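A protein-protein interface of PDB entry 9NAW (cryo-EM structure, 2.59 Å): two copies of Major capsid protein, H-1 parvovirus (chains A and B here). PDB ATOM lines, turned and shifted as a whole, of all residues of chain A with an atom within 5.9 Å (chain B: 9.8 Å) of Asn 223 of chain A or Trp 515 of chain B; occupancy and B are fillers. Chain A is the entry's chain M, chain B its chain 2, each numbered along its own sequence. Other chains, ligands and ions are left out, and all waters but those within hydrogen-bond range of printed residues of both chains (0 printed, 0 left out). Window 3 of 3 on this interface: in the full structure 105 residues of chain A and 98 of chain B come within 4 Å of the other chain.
No position is printed for both chains.
Of the 7 pairs that touch across the chains among the printed residues, none has its exchanged pair printed and touching as well.
O of Phe 218 of chain A lies within hydrogen-bond range of N of Trp 515 of chain B (2.9 Å).
Of chain B, only Trp 515 (3.6 Å) comes within 4 Å of Asn 223 of chain A.
Of chain A, only Phe 218 and Asn 223 come within 4 Å of Trp 515 of chain B.
Of chain B, only Thr 514, Trp 515 and Asn 516 come within 4 Å of Phe 218 of chain A.
No residue of chain B comes within 4 Å of Thr 220 of chain A.
Thr 224 of chain A touches just one residue of chain B: Leu 513 (3.5 Å).
Of the printed residues of chain B, Phe 219 of chain A touches Leu 513 and Thr 514.
Printed residues of chain A within 4 Å of Thr 514 of chain B: Phe 218 (3.7 Å) and Phe 219 (3.7 Å).
Pro 517 of chain B touches none of the printed residues of chain A.
Glu 222 of chain A touches none of the printed residues of chain B.
The nearest printed residue of chain A that does not touch Asn 516 of chain B is Phe 219 of chain A (6.0 Å).
The side-chain hydroxyl (OG1) of Thr 514 of chain B lies within hydrogen-bond range of the backbone carbonyl oxygen (O) of Asn 516 of chain B (3.0 Å).
OG1 of Thr 220 of chain A is in hydrogen-bond range of ND2 of Asn 223 of chain A, 3.1 Å away.
The side-chain hydroxyl (OG1) of Thr 224 of chain A sits at hydrogen-bond distance from the backbone carbonyl oxygen (O) of Thr 220 of chain A (2.8 Å).
Of the 8 printed residues of chain A, 4 touch a printed residue of chain B.
Along chain A the printed residues that touch a printed residue of chain B span positions 218 to 224.
Printed residues of chain B that touch a printed residue of chain A: Leu 513, Thr 514, Trp 515 and Asn 516.
Hydrophobic or aromatic side chains of chain B that line the printed part of chain A: Leu 513 and Trp 515.
Among the printed residues, 7 pairs touch across the chains.
Phe 218 of chain A touches Thr 514 of chain B.
Phe 218 of chain A touches Asn 516 of chain B (N to OD1, 3.7 Å).
CD1 of Phe 219 of chain A touches O of Leu 513 of chain B, 3.7 Å away.
CE1 of Phe 219 of chain A touches CG2 of Thr 514 of chain B, 3.7 Å away.
ND2 of Asn 223 of chain A touches CE3 of Trp 515 of chain B, at 3.6 Å.
Thr 224 of chain A touches Leu 513 of chain B.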
ATOM      1  N   PHE A 218      -4.603  13.649  25.188  1.00  0.00           N
ATOM      2  CA  PHE A 218      -3.396  13.720  25.996  1.00  0.00           C
ATOM      3  C   PHE A 218      -2.286  12.932  25.326  1.00  0.00           C
ATOM      4  O   PHE A 218      -2.426  11.732  25.081  1.00  0.00           O
ATOM      5  CB  PHE A 218      -3.656  13.238  27.422  1.00  0.00           C
ATOM      6  CG  PHE A 218      -2.416  12.966  28.190  1.00  0.00           C
ATOM      7  CD1 PHE A 218      -1.550  13.978  28.514  1.00  0.00           C
ATOM      8  CD2 PHE A 218      -2.173  11.709  28.692  1.00  0.00           C
ATOM      9  CE1 PHE A 218      -0.412  13.719  29.225  1.00  0.00           C
ATOM     10  CE2 PHE A 218      -1.050  11.453  29.424  1.00  0.00           C
ATOM     11  CZ  PHE A 218      -0.169  12.460  29.691  1.00  0.00           C
ATOM     12  N   PHE A 219      -1.195  13.617  25.025  1.00  0.00           N
ATOM     13  CA  PHE A 219      -0.040  13.034  24.377  1.00  0.00           C
ATOM     14  C   PHE A 219       1.128  13.056  25.337  1.00  0.00           C
ATOM     15  O   PHE A 219       1.194  13.882  26.248  1.00  0.00           O
ATOM     16  CB  PHE A 219       0.358  13.791  23.119  1.00  0.00           C
ATOM     17  CG  PHE A 219      -0.674  13.775  22.053  1.00  0.00           C
ATOM     18  CD1 PHE A 219      -0.759  12.718  21.176  1.00  0.00           C
ATOM     19  CD2 PHE A 219      -1.556  14.822  21.922  1.00  0.00           C
ATOM     20  CE1 PHE A 219      -1.709  12.709  20.189  1.00  0.00           C
ATOM     21  CE2 PHE A 219      -2.504  14.816  20.941  1.00  0.00           C
ATOM     22  CZ  PHE A 219      -2.581  13.759  20.074  1.00  0.00           C
ATOM     23  N   THR A 220       2.027  12.085  25.151  1.00  0.00           N
ATOM     24  CA  THR A 220       3.267  12.012  25.962  1.00  0.00           C
ATOM     25  C   THR A 220       4.425  11.840  24.979  1.00  0.00           C
ATOM     26  O   THR A 220       4.232  11.136  23.973  1.00  0.00           O
ATOM     27  CB  THR A 220       3.238  10.851  26.963  1.00  0.00           C
ATOM     28  OG1 THR A 220       3.712   9.679  26.300  1.00  0.00           O
ATOM     29  CG2 THR A 220       1.865  10.594  27.545  1.00  0.00           C
ATOM     30  N   ILE A 221       5.569  12.468  25.246  1.00  0.00           N
ATOM     31  CA  ILE A 221       6.718  12.385  24.352  1.00  0.00           C
ATOM     32  C   ILE A 221       7.170  10.939  24.218  1.00  0.00           C
ATOM     33  O   ILE A 221       7.502  10.475  23.125  1.00  0.00           O
ATOM     34  CB  ILE A 221       7.859  13.277  24.866  1.00  0.00           C
ATOM     35  CG1 ILE A 221       7.388  14.710  25.093  1.00  0.00           C
ATOM     36  CG2 ILE A 221       8.999  13.278  23.885  1.00  0.00           C
ATOM     37  CD1 ILE A 221       6.924  15.401  23.917  1.00  0.00           C
ATOM     38  N   GLU A 222       7.168  10.206  25.327  1.00  0.00           N
ATOM     39  CA  GLU A 222       7.759   8.874  25.349  1.00  0.00           C
ATOM     40  C   GLU A 222       6.988   7.892  24.485  1.00  0.00           C
ATOM     41  O   GLU A 222       7.585   7.029  23.837  1.00  0.00           O
ATOM     42  CB  GLU A 222       7.844   8.374  26.786  1.00  0.00           C
ATOM     43  CG  GLU A 222       8.848   9.118  27.628  1.00  0.00           C
ATOM     44  CD  GLU A 222       8.320  10.424  28.157  1.00  0.00           C
ATOM     45  OE1 GLU A 222       7.189  10.798  27.805  1.00  0.00           O
ATOM     46  OE2 GLU A 222       9.037  11.081  28.931  1.00  0.00           O
ATOM     47  N   ASN A 223       5.665   7.980  24.479  1.00  0.00           N
ATOM     48  CA  ASN A 223       4.898   7.031  23.685  1.00  0.00           C
ATOM     49  C   ASN A 223       4.838   7.418  22.217  1.00  0.00           C
ATOM     50  O   ASN A 223       4.618   6.558  21.363  1.00  0.00           O
ATOM     51  CB  ASN A 223       3.501   6.873  24.251  1.00  0.00           C
ATOM     52  CG  ASN A 223       3.469   6.018  25.489  1.00  0.00           C
ATOM     53  OD1 ASN A 223       3.533   4.799  25.406  1.00  0.00           O
ATOM     54  ND2 ASN A 223       3.371   6.642  26.639  1.00  0.00           N
ATOM     55  N   THR A 224       4.960   8.700  21.899  1.00  0.00           N
ATOM     56  CA  THR A 224       4.800   9.119  20.515  1.00  0.00           C
ATOM     57  C   THR A 224       6.096   9.306  19.739  1.00  0.00           C
ATOM     58  O   THR A 224       6.032   9.497  18.524  1.00  0.00           O
ATOM     59  CB  THR A 224       4.001  10.419  20.464  1.00  0.00           C
ATOM     60  OG1 THR A 224       4.674  11.413  21.238  1.00  0.00           O
ATOM     61  CG2 THR A 224       2.631  10.212  21.030  1.00  0.00           C
ATOM     62  N   LEU A 225       7.261   9.217  20.365  1.00  0.00           N
ATOM     63  CA  LEU A 225       8.463   9.603  19.640  1.00  0.00           C
ATOM     64  C   LEU A 225       9.632   8.698  19.980  1.00  0.00           C
ATOM     65  O   LEU A 225       9.769   8.251  21.120  1.00  0.00           O
ATOM     66  CB  LEU A 225       8.875  11.047  19.951  1.00  0.00           C
ATOM     67  CG  LEU A 225       7.954  12.190  19.540  1.00  0.00           C
ATOM     68  CD1 LEU A 225       8.512  13.506  20.017  1.00  0.00           C
ATOM     69  CD2 LEU A 225       7.778  12.191  18.054  1.00  0.00           C
ATOM     70  N   PRO B 511      -4.747   6.539  12.774  1.00  0.00           N
ATOM     71  CA  PRO B 511      -3.667   6.346  13.741  1.00  0.00           C
ATOM     72  C   PRO B 511      -4.193   6.488  15.153  1.00  0.00           C
ATOM     73  O   PRO B 511      -5.137   7.236  15.414  1.00  0.00           O
ATOM     74  CB  PRO B 511      -2.698   7.479  13.409  1.00  0.00           C
ATOM     75  CG  PRO B 511      -3.584   8.548  12.895  1.00  0.00           C
ATOM     76  CD  PRO B 511      -4.684   7.866  12.144  1.00  0.00           C
ATOM     77  N   ASN B 512      -3.600   5.743  16.074  1.00  0.00           N
ATOM     78  CA  ASN B 512      -3.877   5.951  17.489  1.00  0.00           C
ATOM     79  C   ASN B 512      -2.600   6.408  18.181  1.00  0.00           C
ATOM     80  O   ASN B 512      -1.725   5.591  18.471  1.00  0.00           O
ATOM     81  CB  ASN B 512      -4.397   4.654  18.076  1.00  0.00           C
ATOM     82  CG  ASN B 512      -4.923   4.821  19.443  1.00  0.00           C
ATOM     83  OD1 ASN B 512      -5.451   5.871  19.803  1.00  0.00           O
ATOM     84  ND2 ASN B 512      -4.768   3.788  20.240  1.00  0.00           N
ATOM     85  N   LEU B 513      -2.480   7.707  18.453  1.00  0.00           N
ATOM     86  CA  LEU B 513      -1.348   8.224  19.204  1.00  0.00           C
ATOM     87  C   LEU B 513      -1.611   8.689  20.631  1.00  0.00           C
ATOM     88  O   LEU B 513      -0.649   9.015  21.328  1.00  0.00           O
ATOM     89  CB  LEU B 513      -0.701   9.356  18.398  1.00  0.00           C
ATOM     90  CG  LEU B 513      -0.171   8.682  17.132  1.00  0.00           C
ATOM     91  CD1 LEU B 513       0.301   9.661  16.103  1.00  0.00           C
ATOM     92  CD2 LEU B 513       0.948   7.737  17.503  1.00  0.00           C
ATOM     93  N   THR B 514      -2.853   8.749  21.093  1.00  0.00           N
ATOM     94  CA  THR B 514      -3.107   9.330  22.406  1.00  0.00           C
ATOM     95  C   THR B 514      -2.877   8.322  23.519  1.00  0.00           C
ATOM     96  O   THR B 514      -2.962   7.114  23.315  1.00  0.00           O
ATOM     97  CB  THR B 514      -4.524   9.889  22.516  1.00  0.00           C
ATOM     98  OG1 THR B 514      -5.475   8.850  22.267  1.00  0.00           O
ATOM     99  CG2 THR B 514      -4.727  11.020  21.540  1.00  0.00           C
ATOM    100  N   TRP B 515      -2.578   8.839  24.708  1.00  0.00           N
ATOM    101  CA  TRP B 515      -2.564   7.984  25.886  1.00  0.00           C
ATOM    102  C   TRP B 515      -3.965   7.545  26.258  1.00  0.00           C
ATOM    103  O   TRP B 515      -4.241   6.348  26.371  1.00  0.00           O
ATOM    104  CB  TRP B 515      -1.948   8.713  27.072  1.00  0.00           C
ATOM    105  CG  TRP B 515      -1.993   7.902  28.325  1.00  0.00           C
ATOM    106  CD1 TRP B 515      -2.905   7.998  29.322  1.00  0.00           C
ATOM    107  CD2 TRP B 515      -1.055   6.914  28.737  1.00  0.00           C
ATOM    108  NE1 TRP B 515      -2.621   7.107  30.312  1.00  0.00           N
ATOM    109  CE2 TRP B 515      -1.481   6.431  29.980  1.00  0.00           C
ATOM    110  CE3 TRP B 515       0.098   6.380  28.168  1.00  0.00           C
ATOM    111  CZ2 TRP B 515      -0.796   5.445  30.665  1.00  0.00           C
ATOM    112  CZ3 TRP B 515       0.772   5.405  28.847  1.00  0.00           C
ATOM    113  CH2 TRP B 515       0.328   4.945  30.083  1.00  0.00           C
ATOM    114  N   ASN B 516      -4.861   8.503  26.442  1.00  0.00           N
ATOM    115  CA  ASN B 516      -6.186   8.202  26.930  1.00  0.00           C
ATOM    116  C   ASN B 516      -7.012   7.491  25.866  1.00  0.00           C
ATOM    117  O   ASN B 516      -6.761   7.635  24.670  1.00  0.00           O
ATOM    118  CB  ASN B 516      -6.896   9.480  27.353  1.00  0.00           C
ATOM    119  CG  ASN B 516      -7.014  10.472  26.230  1.00  0.00           C
ATOM    120  OD1 ASN B 516      -6.305  10.389  25.242  1.00  0.00           O
ATOM    121  ND2 ASN B 516      -7.937  11.399  26.361  1.00  0.00           N
ATOM    122  N   PRO B 517      -7.998   6.708  26.282  1.00  0.00           N
ATOM    123  CA  PRO B 517      -8.925   6.121  25.320  1.00  0.00           C
ATOM    124  C   PRO B 517      -9.721   7.187  24.590  1.00  0.00           C
ATOM    125  O   PRO B 517      -9.862   8.318  25.054  1.00  0.00           O
ATOM    126  CB  PRO B 517      -9.821   5.250  26.197  1.00  0.00           C
ATOM    127  CG  PRO B 517      -8.976   4.901  27.329  1.00  0.00           C
ATOM    128  CD  PRO B 517      -8.168   6.115  27.612  1.00  0.00           C
ATOM    129  N   VAL B 518     -10.253   6.807  23.456  1.00  0.00           N
ATOM    130  CA  VAL B 518     -10.871   7.745  22.532  1.00  0.00           C
ATOM    131  C   VAL B 518     -12.378   7.543  22.524  1.00  0.00           C
ATOM    132  O   VAL B 518     -12.881   6.441  22.751  1.00  0.00           O
ATOM    133  CB  VAL B 518     -10.259   7.560  21.130  1.00  0.00           C
ATOM    134  CG1 VAL B 518     -10.950   8.410  20.131  1.00  0.00           C
ATOM    135  CG2 VAL B 518      -8.801   7.914  21.156  1.00  0.00           C
